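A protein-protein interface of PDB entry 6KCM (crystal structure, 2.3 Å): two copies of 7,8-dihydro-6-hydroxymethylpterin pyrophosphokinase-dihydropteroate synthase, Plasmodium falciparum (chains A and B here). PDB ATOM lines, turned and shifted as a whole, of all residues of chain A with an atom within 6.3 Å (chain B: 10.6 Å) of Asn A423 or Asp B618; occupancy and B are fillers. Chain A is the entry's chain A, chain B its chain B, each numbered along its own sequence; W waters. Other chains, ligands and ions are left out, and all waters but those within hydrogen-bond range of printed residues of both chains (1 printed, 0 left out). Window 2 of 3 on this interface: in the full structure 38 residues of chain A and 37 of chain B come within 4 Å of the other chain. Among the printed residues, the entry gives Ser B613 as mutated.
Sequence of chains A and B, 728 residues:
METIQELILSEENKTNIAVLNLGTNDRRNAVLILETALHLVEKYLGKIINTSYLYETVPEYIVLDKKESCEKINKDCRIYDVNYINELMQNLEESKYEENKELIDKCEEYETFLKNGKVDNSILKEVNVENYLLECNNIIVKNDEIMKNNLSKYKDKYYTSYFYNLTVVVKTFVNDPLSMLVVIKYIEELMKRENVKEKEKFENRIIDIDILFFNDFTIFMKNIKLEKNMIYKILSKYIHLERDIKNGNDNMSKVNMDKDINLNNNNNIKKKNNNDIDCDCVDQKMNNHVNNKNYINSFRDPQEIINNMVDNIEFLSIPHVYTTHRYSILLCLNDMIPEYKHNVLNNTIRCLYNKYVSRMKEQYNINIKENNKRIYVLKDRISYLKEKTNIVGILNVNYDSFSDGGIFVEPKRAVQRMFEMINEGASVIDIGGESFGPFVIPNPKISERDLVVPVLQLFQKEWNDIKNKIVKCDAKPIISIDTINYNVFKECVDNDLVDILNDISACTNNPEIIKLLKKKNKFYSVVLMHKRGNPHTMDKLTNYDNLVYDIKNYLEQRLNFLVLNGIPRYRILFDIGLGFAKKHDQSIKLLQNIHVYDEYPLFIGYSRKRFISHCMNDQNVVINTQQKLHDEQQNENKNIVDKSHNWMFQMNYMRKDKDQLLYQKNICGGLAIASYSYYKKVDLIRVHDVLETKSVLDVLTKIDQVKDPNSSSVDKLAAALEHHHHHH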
ATOM      1  N   MET A 418      16.533 -35.433 -17.151  1.00  0.00           N
ATOM      2  CA  MET A 418      17.138 -34.201 -17.665  1.00  0.00           C
ATOM      3  C   MET A 418      16.109 -33.120 -17.998  1.00  0.00           C
ATOM      4  O   MET A 418      16.337 -31.943 -17.733  1.00  0.00           O
ATOM      5  CB  MET A 418      18.015 -34.473 -18.911  1.00  0.00           C
ATOM      6  CG  MET A 418      19.261 -35.296 -18.602  1.00  0.00           C
ATOM      7  SD  MET A 418      20.299 -35.699 -20.015  1.00  0.00           S
ATOM      8  CE  MET A 418      20.914 -34.078 -20.472  1.00  0.00           C
ATOM      9  N   PHE A 419      15.003 -33.515 -18.624  1.00  0.00           N
ATOM     10  CA  PHE A 419      13.924 -32.565 -18.940  1.00  0.00           C
ATOM     11  C   PHE A 419      13.233 -32.110 -17.673  1.00  0.00           C
ATOM     12  O   PHE A 419      12.992 -30.940 -17.497  1.00  0.00           O
ATOM     13  CB  PHE A 419      12.920 -33.160 -19.926  1.00  0.00           C
ATOM     14  CG  PHE A 419      13.352 -33.025 -21.353  1.00  0.00           C
ATOM     15  CD1 PHE A 419      13.145 -31.835 -22.038  1.00  0.00           C
ATOM     16  CD2 PHE A 419      13.993 -34.074 -22.003  1.00  0.00           C
ATOM     17  CE1 PHE A 419      13.555 -31.693 -23.353  1.00  0.00           C
ATOM     18  CE2 PHE A 419      14.413 -33.932 -23.315  1.00  0.00           C
ATOM     19  CZ  PHE A 419      14.195 -32.744 -23.989  1.00  0.00           C
ATOM     20  N   GLU A 420      12.968 -33.046 -16.776  1.00  0.00           N
ATOM     21  CA  GLU A 420      12.406 -32.722 -15.486  1.00  0.00           C
ATOM     22  C   GLU A 420      13.220 -31.614 -14.776  1.00  0.00           C
ATOM     23  O   GLU A 420      12.640 -30.619 -14.328  1.00  0.00           O
ATOM     24  CB  GLU A 420      12.256 -33.995 -14.644  1.00  0.00           C
ATOM     25  CG  GLU A 420      11.790 -33.753 -13.209  1.00  0.00           C
ATOM     26  CD  GLU A 420      11.295 -35.006 -12.491  1.00  0.00           C
ATOM     27  OE1 GLU A 420      11.781 -36.130 -12.778  1.00  0.00           O
ATOM     28  OE2 GLU A 420      10.406 -34.863 -11.618  1.00  0.00           O
ATOM     29  N   MET A 421      14.553 -31.757 -14.722  1.00  0.00           N
ATOM     30  CA  MET A 421      15.411 -30.770 -14.049  1.00  0.00           C
ATOM     31  C   MET A 421      15.407 -29.405 -14.721  1.00  0.00           C
ATOM     32  O   MET A 421      15.473 -28.370 -14.050  1.00  0.00           O
ATOM     33  CB  MET A 421      16.859 -31.295 -13.904  1.00  0.00           C
ATOM     34  CG  MET A 421      17.031 -32.375 -12.837  1.00  0.00           C
ATOM     35  SD  MET A 421      18.750 -32.962 -12.642  1.00  0.00           S
ATOM     36  CE  MET A 421      19.131 -33.494 -14.316  1.00  0.00           C
ATOM     37  N   ILE A 422      15.345 -29.389 -16.048  1.00  0.00           N
ATOM     38  CA  ILE A 422      15.298 -28.121 -16.795  1.00  0.00           C
ATOM     39  C   ILE A 422      14.056 -27.317 -16.406  1.00  0.00           C
ATOM     40  O   ILE A 422      14.141 -26.108 -16.160  1.00  0.00           O
ATOM     41  CB  ILE A 422      15.318 -28.359 -18.326  1.00  0.00           C
ATOM     42  CG1 ILE A 422      16.658 -28.967 -18.758  1.00  0.00           C
ATOM     43  CG2 ILE A 422      15.052 -27.067 -19.116  1.00  0.00           C
ATOM     44  CD1 ILE A 422      16.521 -29.841 -19.991  1.00  0.00           C
ATOM     45  N   ASN A 423      12.910 -27.995 -16.348  1.00  0.00           N
ATOM     46  CA  ASN A 423      11.655 -27.347 -15.979  1.00  0.00           C
ATOM     47  C   ASN A 423      11.659 -26.928 -14.526  1.00  0.00           C
ATOM     48  O   ASN A 423      11.064 -25.912 -14.169  1.00  0.00           O
ATOM     49  CB  ASN A 423      10.468 -28.258 -16.271  1.00  0.00           C
ATOM     50  CG  ASN A 423      10.226 -28.431 -17.761  1.00  0.00           C
ATOM     51  OD1 ASN A 423      10.397 -27.491 -18.557  1.00  0.00           O
ATOM     52  ND2 ASN A 423       9.843 -29.638 -18.151  1.00  0.00           N
ATOM     53  N   GLU A 424      12.357 -27.696 -13.693  1.00  0.00           N
ATOM     54  CA  GLU A 424      12.488 -27.333 -12.295  1.00  0.00           C
ATOM     55  C   GLU A 424      13.426 -26.150 -12.098  1.00  0.00           C
ATOM     56  O   GLU A 424      13.535 -25.646 -10.994  1.00  0.00           O
ATOM     57  CB  GLU A 424      12.958 -28.509 -11.471  1.00  0.00           C
ATOM     58  CG  GLU A 424      11.923 -29.594 -11.257  1.00  0.00           C
ATOM     59  CD  GLU A 424      12.513 -30.812 -10.559  1.00  0.00           C
ATOM     60  OE1 GLU A 424      13.497 -30.681  -9.783  1.00  0.00           O
ATOM     61  OE2 GLU A 424      11.998 -31.920 -10.778  1.00  0.00           O
ATOM     62  N   GLY A 425      14.097 -25.691 -13.152  1.00  0.00           N
ATOM     63  CA  GLY A 425      14.966 -24.500 -13.016  1.00  0.00           C
ATOM     64  C   GLY A 425      16.505 -24.630 -13.100  1.00  0.00           C
ATOM     65  O   GLY A 425      17.219 -23.645 -12.862  1.00  0.00           O
ATOM     66  N   ALA A 426      17.030 -25.808 -13.441  1.00  0.00           N
ATOM     67  CA  ALA A 426      18.488 -25.978 -13.609  1.00  0.00           C
ATOM     68  C   ALA A 426      18.998 -25.230 -14.830  1.00  0.00           C
ATOM     69  O   ALA A 426      18.451 -25.386 -15.924  1.00  0.00           O
ATOM     70  CB  ALA A 426      18.858 -27.462 -13.692  1.00  0.00           C
ATOM     71  N   LYS A 694      15.764 -24.137  -6.244  1.00  0.00           N
ATOM     72  CA  LYS A 694      15.166 -23.053  -6.997  1.00  0.00           C
ATOM     73  C   LYS A 694      14.121 -22.287  -6.171  1.00  0.00           C
ATOM     74  O   LYS A 694      14.037 -21.066  -6.294  1.00  0.00           O
ATOM     75  CB  LYS A 694      14.478 -23.606  -8.252  1.00  0.00           C
ATOM     76  CG  LYS A 694      14.042 -22.530  -9.246  1.00  0.00           C
ATOM     77  CD  LYS A 694      15.217 -21.631  -9.622  1.00  0.00           C
ATOM     78  CE  LYS A 694      14.922 -20.832 -10.891  1.00  0.00           C
ATOM     79  NZ  LYS A 694      13.600 -20.159 -10.789  1.00  0.00           N
ATOM     80  N   ASP A 698      14.536 -18.348  -5.369  1.00  0.00           N
ATOM     81  CA  ASP A 698      13.491 -17.390  -5.794  1.00  0.00           C
ATOM     82  C   ASP A 698      13.042 -16.497  -4.637  1.00  0.00           C
ATOM     83  O   ASP A 698      12.948 -15.284  -4.800  1.00  0.00           O
ATOM     84  CB  ASP A 698      12.305 -18.113  -6.423  1.00  0.00           C
ATOM     85  CG  ASP A 698      12.621 -18.644  -7.826  1.00  0.00           C
ATOM     86  OD1 ASP A 698      13.684 -18.291  -8.401  1.00  0.00           O
ATOM     87  OD2 ASP A 698      11.825 -19.436  -8.357  1.00  0.00           O
ATOM     88  N   SER B 613       4.463 -18.617  -2.221  1.00  0.00           N
ATOM     89  CA  SER B 613       4.183 -19.016  -3.607  1.00  0.00           C
ATOM     90  C   SER B 613       4.272 -17.858  -4.581  1.00  0.00           C
ATOM     91  O   SER B 613       4.730 -18.023  -5.720  1.00  0.00           O
ATOM     92  CB  SER B 613       2.811 -19.687  -3.725  1.00  0.00           C
ATOM     93  OG  SER B 613       2.595 -20.533  -2.590  1.00  0.00           O
ATOM     94  N   HIS B 614       3.862 -16.681  -4.115  1.00  0.00           N
ATOM     95  CA  HIS B 614       3.946 -15.476  -4.918  1.00  0.00           C
ATOM     96  C   HIS B 614       5.374 -15.153  -5.276  1.00  0.00           C
ATOM     97  O   HIS B 614       5.621 -14.469  -6.262  1.00  0.00           O
ATOM     98  CB  HIS B 614       3.285 -14.309  -4.186  1.00  0.00           C
ATOM     99  CG  HIS B 614       3.214 -13.029  -4.984  1.00  0.00           C
ATOM    100  ND1 HIS B 614       4.084 -12.006  -4.798  1.00  0.00           N
ATOM    101  CD2 HIS B 614       2.304 -12.600  -5.966  1.00  0.00           C
ATOM    102  CE1 HIS B 614       3.762 -10.978  -5.623  1.00  0.00           C
ATOM    103  NE2 HIS B 614       2.674 -11.346  -6.344  1.00  0.00           N
ATOM    104  N   CYS B 615       6.340 -15.651  -4.512  1.00  0.00           N
ATOM    105  CA  CYS B 615       7.757 -15.459  -4.907  1.00  0.00           C
ATOM    106  C   CYS B 615       8.266 -16.356  -6.050  1.00  0.00           C
ATOM    107  O   CYS B 615       9.326 -16.079  -6.597  1.00  0.00           O
ATOM    108  CB  CYS B 615       8.682 -15.657  -3.715  1.00  0.00           C
ATOM    109  SG  CYS B 615       8.298 -14.601  -2.322  1.00  0.00           S
ATOM    110  N   MET B 616       7.545 -17.431  -6.364  1.00  0.00           N
ATOM    111  CA  MET B 616       8.007 -18.424  -7.350  1.00  0.00           C
ATOM    112  C   MET B 616       7.713 -18.015  -8.779  1.00  0.00           C
ATOM    113  O   MET B 616       6.655 -17.453  -9.062  1.00  0.00           O
ATOM    114  CB  MET B 616       7.361 -19.797  -7.141  1.00  0.00           C
ATOM    115  CG  MET B 616       7.304 -20.305  -5.721  1.00  0.00           C
ATOM    116  SD  MET B 616       8.930 -20.584  -5.041  1.00  0.00           S
ATOM    117  CE  MET B 616       8.605 -20.732  -3.288  1.00  0.00           C
ATOM    118  N   ASN B 617       8.652 -18.338  -9.670  1.00  0.00           N
ATOM    119  CA  ASN B 617       8.451 -18.262 -11.121  1.00  0.00           C
ATOM    120  C   ASN B 617       8.215 -19.640 -11.764  1.00  0.00           C
ATOM    121  O   ASN B 617       8.146 -20.675 -11.070  1.00  0.00           O
ATOM    122  CB  ASN B 617       9.667 -17.604 -11.783  1.00  0.00           C
ATOM    123  CG  ASN B 617      10.219 -16.451 -10.970  1.00  0.00           C
ATOM    124  OD1 ASN B 617       9.588 -15.400 -10.844  1.00  0.00           O
ATOM    125  ND2 ASN B 617      11.404 -16.645 -10.406  1.00  0.00           N
ATOM    126  N   ASP B 618       8.076 -19.616 -13.094  1.00  0.00           N
ATOM    127  CA  ASP B 618       8.170 -20.783 -13.986  1.00  0.00           C
ATOM    128  C   ASP B 618       8.809 -22.019 -13.333  1.00  0.00           C
ATOM    129  O   ASP B 618       8.641 -23.153 -13.797  1.00  0.00           O
ATOM    130  CB  ASP B 618       8.977 -20.377 -15.235  1.00  0.00           C
ATOM    131  CG  ASP B 618       8.782 -21.331 -16.422  1.00  0.00           C
ATOM    132  OD1 ASP B 618       7.680 -21.902 -16.582  1.00  0.00           O
ATOM    133  OD2 ASP B 618       9.737 -21.491 -17.217  1.00  0.00           O
ATOM    134  N   HIS B 645      11.679 -36.472  -5.730  1.00  0.00           N
ATOM    135  CA  HIS B 645      11.374 -35.525  -4.658  1.00  0.00           C
ATOM    136  C   HIS B 645      11.004 -36.201  -3.372  1.00  0.00           C
ATOM    137  O   HIS B 645      10.122 -37.075  -3.330  1.00  0.00           O
ATOM    138  CB  HIS B 645      10.280 -34.543  -5.078  1.00  0.00           C
ATOM    139  CG  HIS B 645      10.589 -33.812  -6.369  1.00  0.00           C
ATOM    140  ND1 HIS B 645      11.560 -32.880  -6.462  1.00  0.00           N
ATOM    141  CD2 HIS B 645      10.030 -33.921  -7.644  1.00  0.00           C
ATOM    142  CE1 HIS B 645      11.618 -32.417  -7.724  1.00  0.00           C
ATOM    143  NE2 HIS B 645      10.683 -33.053  -8.446  1.00  0.00           N
ATOM    144  N   LYS B 658       0.398 -31.267  -9.546  1.00  0.00           N
ATOM    145  CA  LYS B 658       0.863 -29.879  -9.607  1.00  0.00           C
ATOM    146  C   LYS B 658       0.769 -29.204  -8.234  1.00  0.00           C
ATOM    147  O   LYS B 658       1.619 -28.384  -7.875  1.00  0.00           O
ATOM    148  CB  LYS B 658       0.121 -29.054 -10.680  1.00  0.00           C
ATOM    149  CG  LYS B 658      -0.656 -29.843 -11.741  1.00  0.00           C
ATOM    150  CD  LYS B 658       0.174 -30.862 -12.525  1.00  0.00           C
ATOM    151  CE  LYS B 658      -0.641 -32.133 -12.756  1.00  0.00           C
ATOM    152  NZ  LYS B 658       0.178 -33.278 -13.248  1.00  0.00           N
ATOM    153  N   LEU B 661       3.698 -30.320  -6.034  1.00  0.00           N
ATOM    154  CA  LEU B 661       4.822 -29.469  -6.413  1.00  0.00           C
ATOM    155  C   LEU B 661       4.705 -28.112  -5.738  1.00  0.00           C
ATOM    156  O   LEU B 661       5.641 -27.660  -5.099  1.00  0.00           O
ATOM    157  CB  LEU B 661       4.943 -29.330  -7.940  1.00  0.00           C
ATOM    158  CG  LEU B 661       5.311 -30.651  -8.658  1.00  0.00           C
ATOM    159  CD1 LEU B 661       5.299 -30.539 -10.184  1.00  0.00           C
ATOM    160  CD2 LEU B 661       6.629 -31.235  -8.158  1.00  0.00           C
ATOM    161  N   LEU B 662       3.537 -27.496  -5.831  1.00  0.00           N
ATOM    162  CA  LEU B 662       3.323 -26.189  -5.220  1.00  0.00           C
ATOM    163  C   LEU B 662       3.577 -26.184  -3.703  1.00  0.00           C
ATOM    164  O   LEU B 662       4.262 -25.298  -3.186  1.00  0.00           O
ATOM    165  CB  LEU B 662       1.932 -25.657  -5.571  1.00  0.00           C
ATOM    166  CG  LEU B 662       1.789 -24.666  -6.751  1.00  0.00           C
ATOM    167  CD1 LEU B 662       2.975 -24.628  -7.720  1.00  0.00           C
ATOM    168  CD2 LEU B 662       0.476 -24.890  -7.506  1.00  0.00           C
ATOM    169  N   LYS B 665       7.333 -26.611  -3.054  1.00  0.00           N
ATOM    170  CA  LYS B 665       7.978 -25.329  -3.311  1.00  0.00           C
ATOM    171  C   LYS B 665       7.725 -24.329  -2.176  1.00  0.00           C
ATOM    172  O   LYS B 665       8.610 -23.534  -1.801  1.00  0.00           O
ATOM    173  CB  LYS B 665       7.441 -24.702  -4.582  1.00  0.00           C
ATOM    174  CG  LYS B 665       7.822 -25.370  -5.883  1.00  0.00           C
ATOM    175  CD  LYS B 665       7.581 -24.350  -6.985  1.00  0.00           C
ATOM    176  CE  LYS B 665       7.379 -25.008  -8.327  1.00  0.00           C
ATOM    177  NZ  LYS B 665       7.425 -23.959  -9.390  1.00  0.00           N
HETATM  178  O   HOH W   1      10.267 -21.313  -8.197  1.00  0.00           O
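Of chain B, only Asp B618 comes within 4 Å of Asn A423. Of chain A, only Asn A423 comes within 4 Å of Asp B618. No residue of chain B comes within 4 Å of Ile A422. Glu A424 touches just one residue of chain B: His B645. Of the printed residues of chain A, Cys B615 touches Asp A698. Of the printed residues of chain A, His B645 touches Glu A420 (3.7 Å) and Glu A424 (2.9 Å). Printed residues of chain B within 4 Å of Glu A420: His B645. Met A421 touches none of the printed residues of chain B. The nearest residue of chain B that does not touch Asn A423 is Lys B665 (6.3 Å). The nearest printed residue of chain B that does not touch Glu A420 is Leu B661 (6.3 Å).
O of Phe A419 sits at hydrogen-bond distance from ND2 of Asn A423 (3.5 Å). The side-chain carboxylate (OD1) of Asp A698 is in salt-bridge range of the side-chain amino group (NZ) of Lys A694.
The side-chain carboxylate (OE2) of Glu A424 sits at hydrogen-bond distance from a ring nitrogen (NE2) of His B645, at 2.9 Å. OD1 of Asp A698 lies within hydrogen-bond range of ND2 of Asn B617, 3.5 Å away.
Water W1 lies within hydrogen-bond range of the side-chain carboxylate (OD2) of Asp A698 (2.4 Å) and the side-chain sulfur (SD) of Met B616 (3.5 Å).
No position is printed for both chains. Of the 5 pairs that touch across the chains among the printed residues, none has its exchanged pair printed and touching as well.
Printed residues of chain B that touch a printed residue of chain A: Cys B615, Asn B617, Asp B618 and His B645. Hydrophobic or aromatic side chains of chain B within 4 Å of the printed part of chain A: His B645. Of the 11 printed residues of chain A, 4 touch a printed residue of chain B. Among the printed residues, 5 pairs touch across the chains. Among the printed residues, no Asp or Glu carboxylate lies within 4 Å of a Lys or Arg side-chain nitrogen of the other chain.
Among the printed residues, merely in contact across the chains: Asp A698 with Cys B615 (3.6 Å), Glu A420 with His B645 (3.7 Å) and Asn A423 with Asp B618 (3.7 Å).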
